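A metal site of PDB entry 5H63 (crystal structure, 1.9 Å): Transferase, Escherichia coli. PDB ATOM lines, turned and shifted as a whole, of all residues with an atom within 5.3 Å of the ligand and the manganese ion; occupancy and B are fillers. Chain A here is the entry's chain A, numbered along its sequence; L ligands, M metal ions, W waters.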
ATOM      1  N   GLN A  64      17.164   4.830 -24.250  1.00  0.00           N
ATOM      2  CA  GLN A  64      16.820   6.000 -23.494  1.00  0.00           C
ATOM      3  C   GLN A  64      15.942   6.933 -24.326  1.00  0.00           C
ATOM      4  O   GLN A  64      16.292   7.208 -25.518  1.00  0.00           O
ATOM      5  CB  GLN A  64      18.096   6.735 -23.080  1.00  0.00           C
ATOM      6  CG  GLN A  64      17.842   8.031 -22.269  1.00  0.00           C
ATOM      7  CD  GLN A  64      19.136   8.717 -21.866  1.00  0.00           C
ATOM      8  OE1 GLN A  64      20.100   8.724 -22.595  1.00  0.00           O
ATOM      9  NE2 GLN A  64      19.134   9.282 -20.654  1.00  0.00           N
ATOM     10  N   TRP A  65      14.876   7.472 -23.727  1.00  0.00           N
ATOM     11  CA  TRP A  65      14.129   8.571 -24.360  1.00  0.00           C
ATOM     12  C   TRP A  65      13.696   9.604 -23.304  1.00  0.00           C
ATOM     13  O   TRP A  65      12.737   9.365 -22.557  1.00  0.00           O
ATOM     14  CB  TRP A  65      12.931   8.137 -25.254  1.00  0.00           C
ATOM     15  CG  TRP A  65      12.571   9.252 -26.095  1.00  0.00           C
ATOM     16  CD1 TRP A  65      11.463  10.031 -25.927  1.00  0.00           C
ATOM     17  CD2 TRP A  65      13.318   9.847 -27.138  1.00  0.00           C
ATOM     18  NE1 TRP A  65      11.431  11.036 -26.857  1.00  0.00           N
ATOM     19  CE2 TRP A  65      12.590  10.965 -27.596  1.00  0.00           C
ATOM     20  CE3 TRP A  65      14.562   9.558 -27.734  1.00  0.00           C
ATOM     21  CZ2 TRP A  65      13.048  11.792 -28.634  1.00  0.00           C
ATOM     22  CZ3 TRP A  65      15.025  10.350 -28.752  1.00  0.00           C
ATOM     23  CH2 TRP A  65      14.255  11.485 -29.209  1.00  0.00           C
ATOM     24  N   PHE A  66      14.490  10.679 -23.219  1.00  0.00           N
ATOM     25  CA  PHE A  66      14.178  11.836 -22.391  1.00  0.00           C
ATOM     26  C   PHE A  66      13.474  12.877 -23.267  1.00  0.00           C
ATOM     27  O   PHE A  66      14.005  13.367 -24.268  1.00  0.00           O
ATOM     28  CB  PHE A  66      15.456  12.382 -21.756  1.00  0.00           C
ATOM     29  CG  PHE A  66      15.917  11.643 -20.534  1.00  0.00           C
ATOM     30  CD1 PHE A  66      15.559  10.306 -20.301  1.00  0.00           C
ATOM     31  CD2 PHE A  66      16.643  12.321 -19.541  1.00  0.00           C
ATOM     32  CE1 PHE A  66      15.977   9.612 -19.154  1.00  0.00           C
ATOM     33  CE2 PHE A  66      17.038  11.637 -18.368  1.00  0.00           C
ATOM     34  CZ  PHE A  66      16.697  10.288 -18.182  1.00  0.00           C
ATOM     35  N   GLU A  67      12.263  13.227 -22.885  1.00  0.00           N
ATOM     36  CA  GLU A  67      11.415  13.985 -23.790  1.00  0.00           C
ATOM     37  C   GLU A  67      11.123  15.336 -23.181  1.00  0.00           C
ATOM     38  O   GLU A  67      10.388  15.415 -22.197  1.00  0.00           O
ATOM     39  CB  GLU A  67      10.130  13.191 -24.058  1.00  0.00           C
ATOM     40  CG  GLU A  67       9.135  13.967 -24.931  1.00  0.00           C
ATOM     41  CD  GLU A  67       9.739  14.496 -26.217  1.00  0.00           C
ATOM     42  OE1 GLU A  67       9.718  15.725 -26.430  1.00  0.00           O
ATOM     43  OE2 GLU A  67      10.235  13.710 -27.055  1.00  0.00           O
ATOM     44  N   ARG A  72       4.001  17.520 -27.563  1.00  0.00           N
ATOM     45  CA  ARG A  72       4.032  17.310 -28.996  1.00  0.00           C
ATOM     46  C   ARG A  72       3.486  15.939 -29.481  1.00  0.00           C
ATOM     47  O   ARG A  72       3.253  15.715 -30.674  1.00  0.00           O
ATOM     48  CB  ARG A  72       5.436  17.631 -29.537  1.00  0.00           C
ATOM     49  CG  ARG A  72       6.466  16.506 -29.474  1.00  0.00           C
ATOM     50  CD  ARG A  72       7.874  17.067 -29.643  1.00  0.00           C
ATOM     51  NE  ARG A  72       8.877  16.036 -29.317  1.00  0.00           N
ATOM     52  CZ  ARG A  72       9.807  15.554 -30.128  1.00  0.00           C
ATOM     53  NH1 ARG A  72       9.956  16.025 -31.366  1.00  0.00           N
ATOM     54  NH2 ARG A  72      10.632  14.596 -29.660  1.00  0.00           N
ATOM     55  N   ASN A  86      13.503   9.811 -37.804  1.00  0.00           N
ATOM     56  CA  ASN A  86      13.923   9.288 -36.471  1.00  0.00           C
ATOM     57  C   ASN A  86      12.907   8.222 -35.993  1.00  0.00           C
ATOM     58  O   ASN A  86      12.070   8.520 -35.147  1.00  0.00           O
ATOM     59  CB  ASN A  86      14.018  10.426 -35.463  1.00  0.00           C
ATOM     60  CG  ASN A  86      15.128  11.426 -35.796  1.00  0.00           C
ATOM     61  OD1 ASN A  86      14.823  12.582 -36.016  1.00  0.00           O
ATOM     62  ND2 ASN A  86      16.364  10.987 -35.845  1.00  0.00           N
ATOM     63  N   TYR A  88      12.486   5.985 -33.905  1.00  0.00           N
ATOM     64  CA  TYR A  88      13.135   5.373 -32.717  1.00  0.00           C
ATOM     65  C   TYR A  88      12.324   4.351 -31.928  1.00  0.00           C
ATOM     66  O   TYR A  88      12.849   3.321 -31.524  1.00  0.00           O
ATOM     67  CB  TYR A  88      13.788   6.445 -31.867  1.00  0.00           C
ATOM     68  CG  TYR A  88      14.967   7.209 -32.500  1.00  0.00           C
ATOM     69  CD1 TYR A  88      15.488   6.879 -33.751  1.00  0.00           C
ATOM     70  CD2 TYR A  88      15.540   8.295 -31.852  1.00  0.00           C
ATOM     71  CE1 TYR A  88      16.573   7.551 -34.314  1.00  0.00           C
ATOM     72  CE2 TYR A  88      16.655   8.942 -32.384  1.00  0.00           C
ATOM     73  CZ  TYR A  88      17.124   8.596 -33.670  1.00  0.00           C
ATOM     74  OH  TYR A  88      18.191   9.304 -34.225  1.00  0.00           O
ATOM     75  N   HIS A 200      21.089  18.373 -24.571  1.00  0.00           N
ATOM     76  CA  HIS A 200      21.618  17.011 -24.581  1.00  0.00           C
ATOM     77  C   HIS A 200      22.284  16.613 -23.262  1.00  0.00           C
ATOM     78  O   HIS A 200      22.384  15.436 -22.958  1.00  0.00           O
ATOM     79  CB  HIS A 200      22.605  16.753 -25.735  1.00  0.00           C
ATOM     80  CG  HIS A 200      23.895  17.477 -25.595  1.00  0.00           C
ATOM     81  ND1 HIS A 200      25.000  16.910 -25.023  1.00  0.00           N
ATOM     82  CD2 HIS A 200      24.226  18.763 -25.849  1.00  0.00           C
ATOM     83  CE1 HIS A 200      25.970  17.808 -24.978  1.00  0.00           C
ATOM     84  NE2 HIS A 200      25.532  18.937 -25.479  1.00  0.00           N
ATOM     85  N   PHE A 203      19.941  14.165 -20.909  1.00  0.00           N
ATOM     86  CA  PHE A 203      20.018  12.705 -21.150  1.00  0.00           C
ATOM     87  C   PHE A 203      21.430  12.150 -21.023  1.00  0.00           C
ATOM     88  O   PHE A 203      21.597  11.061 -20.454  1.00  0.00           O
ATOM     89  CB  PHE A 203      19.299  12.219 -22.404  1.00  0.00           C
ATOM     90  CG  PHE A 203      19.483  13.050 -23.628  1.00  0.00           C
ATOM     91  CD1 PHE A 203      18.566  14.028 -23.948  1.00  0.00           C
ATOM     92  CD2 PHE A 203      20.467  12.757 -24.508  1.00  0.00           C
ATOM     93  CE1 PHE A 203      18.676  14.747 -25.144  1.00  0.00           C
ATOM     94  CE2 PHE A 203      20.595  13.418 -25.710  1.00  0.00           C
ATOM     95  CZ  PHE A 203      19.717  14.432 -26.039  1.00  0.00           C
ATOM     96  N   ASP A 204      22.445  12.864 -21.470  1.00  0.00           N
ATOM     97  CA  ASP A 204      23.830  12.338 -21.365  1.00  0.00           C
ATOM     98  C   ASP A 204      24.281  12.100 -19.923  1.00  0.00           C
ATOM     99  O   ASP A 204      24.893  11.066 -19.613  1.00  0.00           O
ATOM    100  CB  ASP A 204      24.840  13.196 -22.113  1.00  0.00           C
ATOM    101  CG  ASP A 204      24.699  13.079 -23.600  1.00  0.00           C
ATOM    102  OD1 ASP A 204      23.863  12.253 -24.075  1.00  0.00           O
ATOM    103  OD2 ASP A 204      25.388  13.846 -24.272  1.00  0.00           O
ATOM    104  N   ARG A 207      22.154   9.174 -18.331  1.00  0.00           N
ATOM    105  CA  ARG A 207      22.580   7.872 -18.912  1.00  0.00           C
ATOM    106  C   ARG A 207      23.743   7.261 -18.103  1.00  0.00           C
ATOM    107  O   ARG A 207      23.702   6.088 -17.748  1.00  0.00           O
ATOM    108  CB  ARG A 207      22.907   8.071 -20.400  1.00  0.00           C
ATOM    109  CG  ARG A 207      23.367   6.807 -21.110  1.00  0.00           C
ATOM    110  CD  ARG A 207      23.771   7.148 -22.513  1.00  0.00           C
ATOM    111  NE  ARG A 207      22.742   7.919 -23.218  1.00  0.00           N
ATOM    112  CZ  ARG A 207      22.953   8.585 -24.351  1.00  0.00           C
ATOM    113  NH1 ARG A 207      24.152   8.692 -24.884  1.00  0.00           N
ATOM    114  NH2 ARG A 207      21.929   9.271 -24.897  1.00  0.00           N
ATOM    115  N   TYR A 237      23.825  -0.355 -22.993  1.00  0.00           N
ATOM    116  CA  TYR A 237      23.170   0.866 -23.451  1.00  0.00           C
ATOM    117  C   TYR A 237      23.403   1.073 -24.941  1.00  0.00           C
ATOM    118  O   TYR A 237      24.594   1.051 -25.394  1.00  0.00           O
ATOM    119  CB  TYR A 237      23.709   2.105 -22.704  1.00  0.00           C
ATOM    120  CG  TYR A 237      23.150   3.285 -23.370  1.00  0.00           C
ATOM    121  CD1 TYR A 237      21.852   3.674 -23.141  1.00  0.00           C
ATOM    122  CD2 TYR A 237      23.871   3.907 -24.397  1.00  0.00           C
ATOM    123  CE1 TYR A 237      21.297   4.702 -23.897  1.00  0.00           C
ATOM    124  CE2 TYR A 237      23.324   4.908 -25.162  1.00  0.00           C
ATOM    125  CZ  TYR A 237      22.038   5.322 -24.892  1.00  0.00           C
ATOM    126  OH  TYR A 237      21.474   6.329 -25.681  1.00  0.00           O
ATOM    127  N   LEU A 238      22.331   1.373 -25.650  1.00  0.00           N
ATOM    128  CA  LEU A 238      22.366   1.718 -27.105  1.00  0.00           C
ATOM    129  C   LEU A 238      21.524   2.929 -27.381  1.00  0.00           C
ATOM    130  O   LEU A 238      20.343   2.987 -26.929  1.00  0.00           O
ATOM    131  CB  LEU A 238      21.823   0.576 -27.969  1.00  0.00           C
ATOM    132  CG  LEU A 238      22.456  -0.770 -27.874  1.00  0.00           C
ATOM    133  CD1 LEU A 238      21.584  -1.734 -28.653  1.00  0.00           C
ATOM    134  CD2 LEU A 238      23.867  -0.889 -28.357  1.00  0.00           C
ATOM    135  N   ASP A 239      22.071   3.854 -28.144  1.00  0.00           N
ATOM    136  CA  ASP A 239      21.284   4.876 -28.840  1.00  0.00           C
ATOM    137  C   ASP A 239      20.201   4.155 -29.703  1.00  0.00           C
ATOM    138  O   ASP A 239      20.455   3.118 -30.297  1.00  0.00           O
ATOM    139  CB  ASP A 239      22.169   5.717 -29.770  1.00  0.00           C
ATOM    140  CG  ASP A 239      22.973   6.825 -29.045  1.00  0.00           C
ATOM    141  OD1 ASP A 239      22.836   7.018 -27.799  1.00  0.00           O
ATOM    142  OD2 ASP A 239      23.717   7.564 -29.741  1.00  0.00           O
ATOM    143  N   ALA A 240      19.032   4.747 -29.814  1.00  0.00           N
ATOM    144  CA  ALA A 240      17.898   4.142 -30.492  1.00  0.00           C
ATOM    145  C   ALA A 240      18.064   4.007 -31.997  1.00  0.00           C
ATOM    146  O   ALA A 240      17.293   3.314 -32.607  1.00  0.00           O
ATOM    147  CB  ALA A 240      16.622   4.910 -30.149  1.00  0.00           C
ATOM    148  N   ASP A 241      19.098   4.618 -32.592  1.00  0.00           N
ATOM    149  CA  ASP A 241      19.428   4.402 -34.000  1.00  0.00           C
ATOM    150  C   ASP A 241      20.546   3.341 -34.242  1.00  0.00           C
ATOM    151  O   ASP A 241      21.053   3.256 -35.360  1.00  0.00           O
ATOM    152  CB  ASP A 241      19.852   5.743 -34.579  1.00  0.00           C
ATOM    153  CG  ASP A 241      21.244   6.213 -34.052  1.00  0.00           C
ATOM    154  OD1 ASP A 241      21.756   5.694 -33.012  1.00  0.00           O
ATOM    155  OD2 ASP A 241      21.756   7.165 -34.652  1.00  0.00           O
ATOM    156  N   MET A 242      20.975   2.637 -33.200  1.00  0.00           N
ATOM    157  CA  MET A 242      21.895   1.532 -33.297  1.00  0.00           C
ATOM    158  C   MET A 242      21.014   0.296 -33.646  1.00  0.00           C
ATOM    159  O   MET A 242      20.392  -0.329 -32.778  1.00  0.00           O
ATOM    160  CB  MET A 242      22.645   1.330 -31.940  1.00  0.00           C
ATOM    161  CG  MET A 242      23.461   2.513 -31.457  1.00  0.00           C
ATOM    162  SD  MET A 242      24.984   2.653 -32.380  1.00  0.00           S
ATOM    163  CE  MET A 242      25.756   4.155 -31.727  1.00  0.00           C
ATOM    164  N   HIS A 260      31.240   2.731 -27.745  1.00  0.00           N
ATOM    165  CA  HIS A 260      31.255   3.037 -29.158  1.00  0.00           C
ATOM    166  C   HIS A 260      32.549   3.788 -29.576  1.00  0.00           C
ATOM    167  O   HIS A 260      33.032   4.698 -28.844  1.00  0.00           O
ATOM    168  CB  HIS A 260      30.005   3.874 -29.513  1.00  0.00           C
ATOM    169  CG  HIS A 260      29.846   4.206 -30.952  1.00  0.00           C
ATOM    170  ND1 HIS A 260      30.018   3.301 -31.973  1.00  0.00           N
ATOM    171  CD2 HIS A 260      29.405   5.349 -31.533  1.00  0.00           C
ATOM    172  CE1 HIS A 260      29.733   3.885 -33.130  1.00  0.00           C
ATOM    173  NE2 HIS A 260      29.356   5.138 -32.882  1.00  0.00           N
ATOM    174  N   GLU A 271      33.139   7.607 -28.540  1.00  0.00           N
ATOM    175  CA  GLU A 271      31.838   8.246 -28.714  1.00  0.00           C
ATOM    176  C   GLU A 271      30.931   7.724 -27.681  1.00  0.00           C
ATOM    177  O   GLU A 271      31.104   6.654 -27.162  1.00  0.00           O
ATOM    178  CB  GLU A 271      31.256   7.923 -30.069  1.00  0.00           C
ATOM    179  CG  GLU A 271      32.105   8.401 -31.228  1.00  0.00           C
ATOM    180  CD  GLU A 271      32.214   9.896 -31.351  1.00  0.00           C
ATOM    181  OE1 GLU A 271      32.979  10.286 -32.227  1.00  0.00           O
ATOM    182  OE2 GLU A 271      31.602  10.684 -30.624  1.00  0.00           O
ATOM    183  N   ASN A 272      29.943   8.535 -27.387  1.00  0.00           N
ATOM    184  CA  ASN A 272      28.842   8.099 -26.661  1.00  0.00           C
ATOM    185  C   ASN A 272      28.021   7.216 -27.623  1.00  0.00           C
ATOM    186  O   ASN A 272      28.214   7.280 -28.859  1.00  0.00           O
ATOM    187  CB  ASN A 272      28.071   9.340 -26.195  1.00  0.00           C
ATOM    188  CG  ASN A 272      27.362   9.068 -24.913  1.00  0.00           C
ATOM    189  OD1 ASN A 272      26.942   7.896 -24.677  1.00  0.00           O
ATOM    190  ND2 ASN A 272      27.140  10.098 -24.132  1.00  0.00           N
ATOM    191  N   GLY A 273      27.078   6.494 -27.109  1.00  0.00           N
ATOM    192  CA  GLY A 273      26.045   5.916 -27.976  1.00  0.00           C
ATOM    193  C   GLY A 273      25.957   4.414 -27.891  1.00  0.00           C
ATOM    194  O   GLY A 273      24.932   3.847 -28.262  1.00  0.00           O
ATOM    195  N   ASN A 338      24.737   4.109 -35.333  1.00  0.00           N
ATOM    196  CA  ASN A 338      24.604   5.576 -35.500  1.00  0.00           C
ATOM    197  C   ASN A 338      23.931   5.901 -36.845  1.00  0.00           C
ATOM    198  O   ASN A 338      24.446   6.707 -37.647  1.00  0.00           O
ATOM    199  CB  ASN A 338      25.973   6.306 -35.374  1.00  0.00           C
ATOM    200  CG  ASN A 338      25.821   7.809 -35.282  1.00  0.00           C
ATOM    201  OD1 ASN A 338      24.713   8.328 -35.187  1.00  0.00           O
ATOM    202  ND2 ASN A 338      26.932   8.529 -35.328  1.00  0.00           N
ATOM    203  N   THR A 339      22.780   5.285 -37.079  1.00  0.00           N
ATOM    204  CA  THR A 339      22.093   5.515 -38.363  1.00  0.00           C
ATOM    205  C   THR A 339      21.520   6.906 -38.538  1.00  0.00           C
ATOM    206  O   THR A 339      21.233   7.322 -39.665  1.00  0.00           O
ATOM    207  CB  THR A 339      21.019   4.463 -38.657  1.00  0.00           C
ATOM    208  OG1 THR A 339      19.984   4.496 -37.668  1.00  0.00           O
ATOM    209  CG2 THR A 339      21.618   3.102 -38.749  1.00  0.00           C
ATOM    210  N   SER A 340      21.392   7.658 -37.473  1.00  0.00           N
ATOM    211  CA  SER A 340      20.972   9.038 -37.589  1.00  0.00           C
ATOM    212  C   SER A 340      21.969   9.896 -38.418  1.00  0.00           C
ATOM    213  O   SER A 340      21.578  10.803 -39.041  1.00  0.00           O
ATOM    214  CB  SER A 340      20.765   9.667 -36.224  1.00  0.00           C
ATOM    215  OG  SER A 340      21.926  10.119 -35.703  1.00  0.00           O
ATOM    216  N   SER A 341      23.251   9.593 -38.381  1.00  0.00           N
ATOM    217  CA  SER A 341      24.237  10.380 -39.103  1.00  0.00           C
ATOM    218  C   SER A 341      24.115  10.204 -40.597  1.00  0.00           C
ATOM    219  O   SER A 341      24.752  10.877 -41.341  1.00  0.00           O
ATOM    220  CB  SER A 341      25.641  10.163 -38.612  1.00  0.00           C
ATOM    221  OG  SER A 341      26.003   8.863 -38.731  1.00  0.00           O
ATOM    222  N   ALA A 344      18.983  12.077 -39.903  1.00  0.00           N
ATOM    223  CA  ALA A 344      19.069  13.306 -39.103  1.00  0.00           C
ATOM    224  C   ALA A 344      19.080  13.135 -37.598  1.00  0.00           C
ATOM    225  O   ALA A 344      18.306  12.419 -37.039  1.00  0.00           O
ATOM    226  CB  ALA A 344      17.983  14.301 -39.468  1.00  0.00           C
ATOM    227  N   SER A 345      19.899  13.951 -36.967  1.00  0.00           N
ATOM    228  CA  SER A 345      20.007  14.014 -35.486  1.00  0.00           C
ATOM    229  C   SER A 345      18.658  14.406 -34.860  1.00  0.00           C
ATOM    230  O   SER A 345      18.004  15.384 -35.280  1.00  0.00           O
ATOM    231  CB  SER A 345      21.069  15.062 -35.089  1.00  0.00           C
ATOM    232  OG  SER A 345      22.016  14.548 -34.167  1.00  0.00           O
ATOM    233  N   SER A 346      18.250  13.651 -33.832  1.00  0.00           N
ATOM    234  CA  SER A 346      16.969  13.900 -33.152  1.00  0.00           C
ATOM    235  C   SER A 346      16.968  15.155 -32.258  1.00  0.00           C
ATOM    236  O   SER A 346      15.911  15.480 -31.737  1.00  0.00           O
ATOM    237  CB  SER A 346      16.655  12.712 -32.265  1.00  0.00           C
ATOM    238  OG  SER A 346      17.759  12.513 -31.445  1.00  0.00           O
ATOM    239  N   TRP A 347      18.137  15.793 -32.031  1.00  0.00           N
ATOM    240  CA  TRP A 347      18.289  16.972 -31.112  1.00  0.00           C
ATOM    241  C   TRP A 347      19.285  18.102 -31.551  1.00  0.00           C
ATOM    242  O   TRP A 347      19.381  19.110 -30.861  1.00  0.00           O
ATOM    243  CB  TRP A 347      18.730  16.480 -29.708  1.00  0.00           C
ATOM    244  CG  TRP A 347      20.112  15.930 -29.792  1.00  0.00           C
ATOM    245  CD1 TRP A 347      20.475  14.682 -30.194  1.00  0.00           C
ATOM    246  CD2 TRP A 347      21.315  16.677 -29.628  1.00  0.00           C
ATOM    247  NE1 TRP A 347      21.823  14.581 -30.250  1.00  0.00           N
ATOM    248  CE2 TRP A 347      22.379  15.793 -29.912  1.00  0.00           C
ATOM    249  CE3 TRP A 347      21.610  18.016 -29.255  1.00  0.00           C
ATOM    250  CZ2 TRP A 347      23.722  16.185 -29.804  1.00  0.00           C
ATOM    251  CZ3 TRP A 347      22.949  18.398 -29.164  1.00  0.00           C
ATOM    252  CH2 TRP A 347      23.997  17.474 -29.431  1.00  0.00           C
ATOM    253  N   ARG A 348      20.029  17.941 -32.644  1.00  0.00           N
ATOM    254  CA  ARG A 348      21.056  18.964 -33.015  1.00  0.00           C
ATOM    255  C   ARG A 348      20.458  20.165 -33.777  1.00  0.00           C
ATOM    256  O   ARG A 348      19.741  20.007 -34.772  1.00  0.00           O
ATOM    257  CB  ARG A 348      22.237  18.336 -33.787  1.00  0.00           C
ATOM    258  CG  ARG A 348      23.128  17.451 -32.914  1.00  0.00           C
ATOM    259  CD  ARG A 348      24.234  16.775 -33.732  1.00  0.00           C
ATOM    260  NE  ARG A 348      24.863  15.661 -33.007  1.00  0.00           N
ATOM    261  CZ  ARG A 348      25.805  15.771 -32.061  1.00  0.00           C
ATOM    262  NH1 ARG A 348      26.234  16.975 -31.657  1.00  0.00           N
ATOM    263  NH2 ARG A 348      26.280  14.675 -31.469  1.00  0.00           N
HETATM  264  C1  LIG L   1      24.934  11.650 -30.201  1.00  0.00           C
HETATM  265  C2  LIG L   1      25.471  10.427 -29.396  1.00  0.00           C
HETATM  266  C3  LIG L   1      24.499  10.112 -28.264  1.00  0.00           C
HETATM  267  C4  LIG L   1      24.467  11.364 -27.407  1.00  0.00           C
HETATM  268  C5  LIG L   1      24.039  12.577 -28.262  1.00  0.00           C
HETATM  269  C6  LIG L   1      23.970  13.859 -27.424  1.00  0.00           C
HETATM  270  C7  LIG L   1      26.779   9.023 -31.026  1.00  0.00           C
HETATM  271  C8  LIG L   1      27.778  10.081 -31.097  1.00  0.00           C
HETATM  272  N1  LIG L   1      25.745   9.251 -30.249  1.00  0.00           N
HETATM  273  O1  LIG L   1      23.616  11.408 -30.755  1.00  0.00           O
HETATM  274  O2  LIG L   1      24.899   8.970 -27.503  1.00  0.00           O
HETATM  275  O3  LIG L   1      23.448  11.321 -26.436  1.00  0.00           O
HETATM  276  O4  LIG L   1      24.960  12.775 -29.321  1.00  0.00           O
HETATM  277  O5  LIG L   1      25.263  14.148 -26.988  1.00  0.00           O
HETATM  278  O6  LIG L   1      26.900   7.943 -31.723  1.00  0.00           O
HETATM  279  N2  LIG L   1      17.867  11.562 -27.037  1.00  0.00           N
HETATM  280  C9  LIG L   1      16.877  11.832 -26.070  1.00  0.00           C
HETATM  281  N3  LIG L   1      15.996  12.812 -26.233  1.00  0.00           N
HETATM  282  C10 LIG L   1      16.049  13.584 -27.336  1.00  0.00           C
HETATM  283  C11 LIG L   1      17.014  13.362 -28.313  1.00  0.00           C
HETATM  284  C12 LIG L   1      17.936  12.329 -28.154  1.00  0.00           C
HETATM  285  O7  LIG L   1      16.793  11.096 -25.039  1.00  0.00           O
HETATM  286  O8  LIG L   1      15.237  14.527 -27.437  1.00  0.00           O
HETATM  287  C13 LIG L   1      18.803  10.461 -26.757  1.00  0.00           C
HETATM  288  C14 LIG L   1      18.230   9.120 -27.156  1.00  0.00           C
HETATM  289  O9  LIG L   1      18.644   8.169 -26.201  1.00  0.00           O
HETATM  290  C15 LIG L   1      18.829   8.883 -28.534  1.00  0.00           C
HETATM  291  C16 LIG L   1      20.174   9.539 -28.345  1.00  0.00           C
HETATM  292  O10 LIG L   1      19.968  10.678 -27.478  1.00  0.00           O
HETATM  293  O11 LIG L   1      19.053   7.523 -28.805  1.00  0.00           O
HETATM  294  C17 LIG L   1      20.877   9.897 -29.617  1.00  0.00           C
HETATM  295  O12 LIG L   1      20.040  10.569 -30.558  1.00  0.00           O
HETATM  296  P1  LIG L   1      20.662  10.604 -32.033  1.00  0.00           P
HETATM  297  O13 LIG L   1      19.491  11.101 -32.796  1.00  0.00           O
HETATM  298  O14 LIG L   1      21.298   9.309 -32.391  1.00  0.00           O
HETATM  299  O15 LIG L   1      21.748  11.795 -32.054  1.00  0.00           O
HETATM  300  P2  LIG L   1      23.314  11.735 -32.329  1.00  0.00           P
HETATM  301  O16 LIG L   1      23.881  10.624 -33.066  1.00  0.00           O
HETATM  302  O17 LIG L   1      23.858  13.070 -32.495  1.00  0.00           O
HETATM  303 MN    MN M   1      22.917   8.839 -33.842  1.00  0.00          MN
HETATM  304  O   HOH W   1      18.744   5.147 -26.582  1.00  0.00           O
HETATM  305  O   HOH W   2      19.515   7.301 -31.618  1.00  0.00           O
HETATM  306  O   HOH W   3      14.254  15.396 -29.775  1.00  0.00           O
HETATM  307  O   HOH W   4      23.649   7.436 -32.480  1.00  0.00           O
HETATM  308  O   HOH W   5      27.754  12.462 -25.235  1.00  0.00           O
HETATM  309  O   HOH W   6      26.201  11.236 -34.684  1.00  0.00           O
HETATM  310  O   HOH W   7      13.710  16.303 -25.739  1.00  0.00           O
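An oxygen (O5) of the ligand sits at hydrogen-bond distance from a ring nitrogen (ND1) of His 200, at 3.4 Å.
N of Ala 240 lies within hydrogen-bond range of O11 of the ligand, 3.0 Å away.
An oxygen (O9) of the ligand is in hydrogen-bond range of the backbone carbonyl oxygen of Gln 64, 2.6 Å away.
A nitrogen (N1) of the ligand is in hydrogen-bond range of the side-chain carboxylate (OD2) of Asp 239 (2.7 Å).
An oxygen (O13) of the ligand sits at hydrogen-bond distance from the side-chain hydroxyl (OH) of Tyr 88 (2.6 Å).
The backbone NH of Gly 273 lies close to an oxygen (O2) of the ligand (3.3 Å).
An oxygen (O13) of the ligand lies within hydrogen-bond range of the side-chain hydroxyl (OG) of Ser 346, at 2.6 Å.
NE1 of Trp 347 lies within hydrogen-bond range of O15 of the ligand, at 3.3 Å.
NH1 of Arg 207 lies within hydrogen-bond range of O2 of the ligand, 2.7 Å away.
The backbone NH of Phe 66 sits at hydrogen-bond distance from an oxygen (O7) of the ligand (3.0 Å).
The backbone carbonyl oxygen (O) of Phe 66 sits at hydrogen-bond distance from a nitrogen (N3) of the ligand (2.9 Å).
O9 of the ligand lies within hydrogen-bond range of OH of Tyr 237, at 3.4 Å.
The backbone NH of Ser 346 lies within hydrogen-bond range of an oxygen (O13) of the ligand (3.0 Å).
N1 of the ligand sits close to O of Asn 272.
NE of Arg 348 lies within salt-bridge range of O17 of the ligand, at 2.8 Å.
OD1 of Asp 204 sits at hydrogen-bond distance from O3 of the ligand (2.6 Å).
The side-chain hydroxyl (OG) of Ser 345 is in hydrogen-bond range of an oxygen (O17) of the ligand.
The backbone NH (N) of Asn 338 lies within hydrogen-bond range of the side-chain sulfur (SD) of Met 242 (3.3 Å).
O of Asn 338 is in hydrogen-bond range of OG of Ser 341 (2.9 Å).
N of Asp 239 lies within hydrogen-bond range of O of Gly 273.
The side-chain carboxylate of Asp 239 is in hydrogen-bond range of the side-chain hydroxyl of Tyr 237 (2.6 Å).
The guanidinium group (NH2) of Arg 207 lies within salt-bridge range of the side-chain carboxylate (OD1) of Asp 204, 3.6 Å away.
NE2 of Gln 64 lies within hydrogen-bond range of O of Phe 203.
The backbone carbonyl oxygen of His 260 lies within hydrogen-bond range of the backbone NH of Glu 271 (2.9 Å).
OG of Ser 345 lies close to NE of Arg 348, at 3.3 Å.
Residues that only touch the ligand: Phe 203, Trp 65, His 260, Glu 271 and Met 242.
Of the 30 residues printed, 23 come within 4 Å of the ligand.
Along chain A the residues within 4 Å of the ligand span positions 64 to 348.
The nearest printed residue that does not touch the manganese ion is Asp 239 (4.4 Å).
Water W4 is bound to the manganese ion (2.1 Å).
O16 of the ligand is bound to the manganese ion (2.2 Å).
OD2 of Asp 241 binds the manganese ion, at 2.2 Å.
The manganese ion is bound by an oxygen (O14) of the ligand, 2.2 Å away.
OD1 of Asn 338 is bound to the manganese ion, 2.3 Å away.
OG of Ser 340 is bound to the manganese ion.
Water W3 bridges the backbone carbonyl oxygen of Ser 346 (2.6 Å) and an oxygen (O8) of the ligand (2.7 Å).
Water W2 lies within hydrogen-bond range of an oxygen (O11) of the ligand (2.9 Å), the backbone NH of Asp 241 (2.9 Å) and the backbone NH of Ala 240 (3.2 Å).
Water W7 lies within hydrogen-bond range of an oxygen (O8) of the ligand and the backbone carbonyl oxygen (O) of Phe 66.
Water W1 lies within hydrogen-bond range of the backbone carbonyl oxygen of Leu 238, the backbone NH of Gln 64, an oxygen (O9) of the ligand, the side-chain hydroxyl of Tyr 237 and the backbone NH of Ala 240.
Water W5 lies within hydrogen-bond range of ND2 of Asn 272 (2.7 Å), OD2 of Asp 204 (2.9 Å) and O5 of the ligand (3.5 Å).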
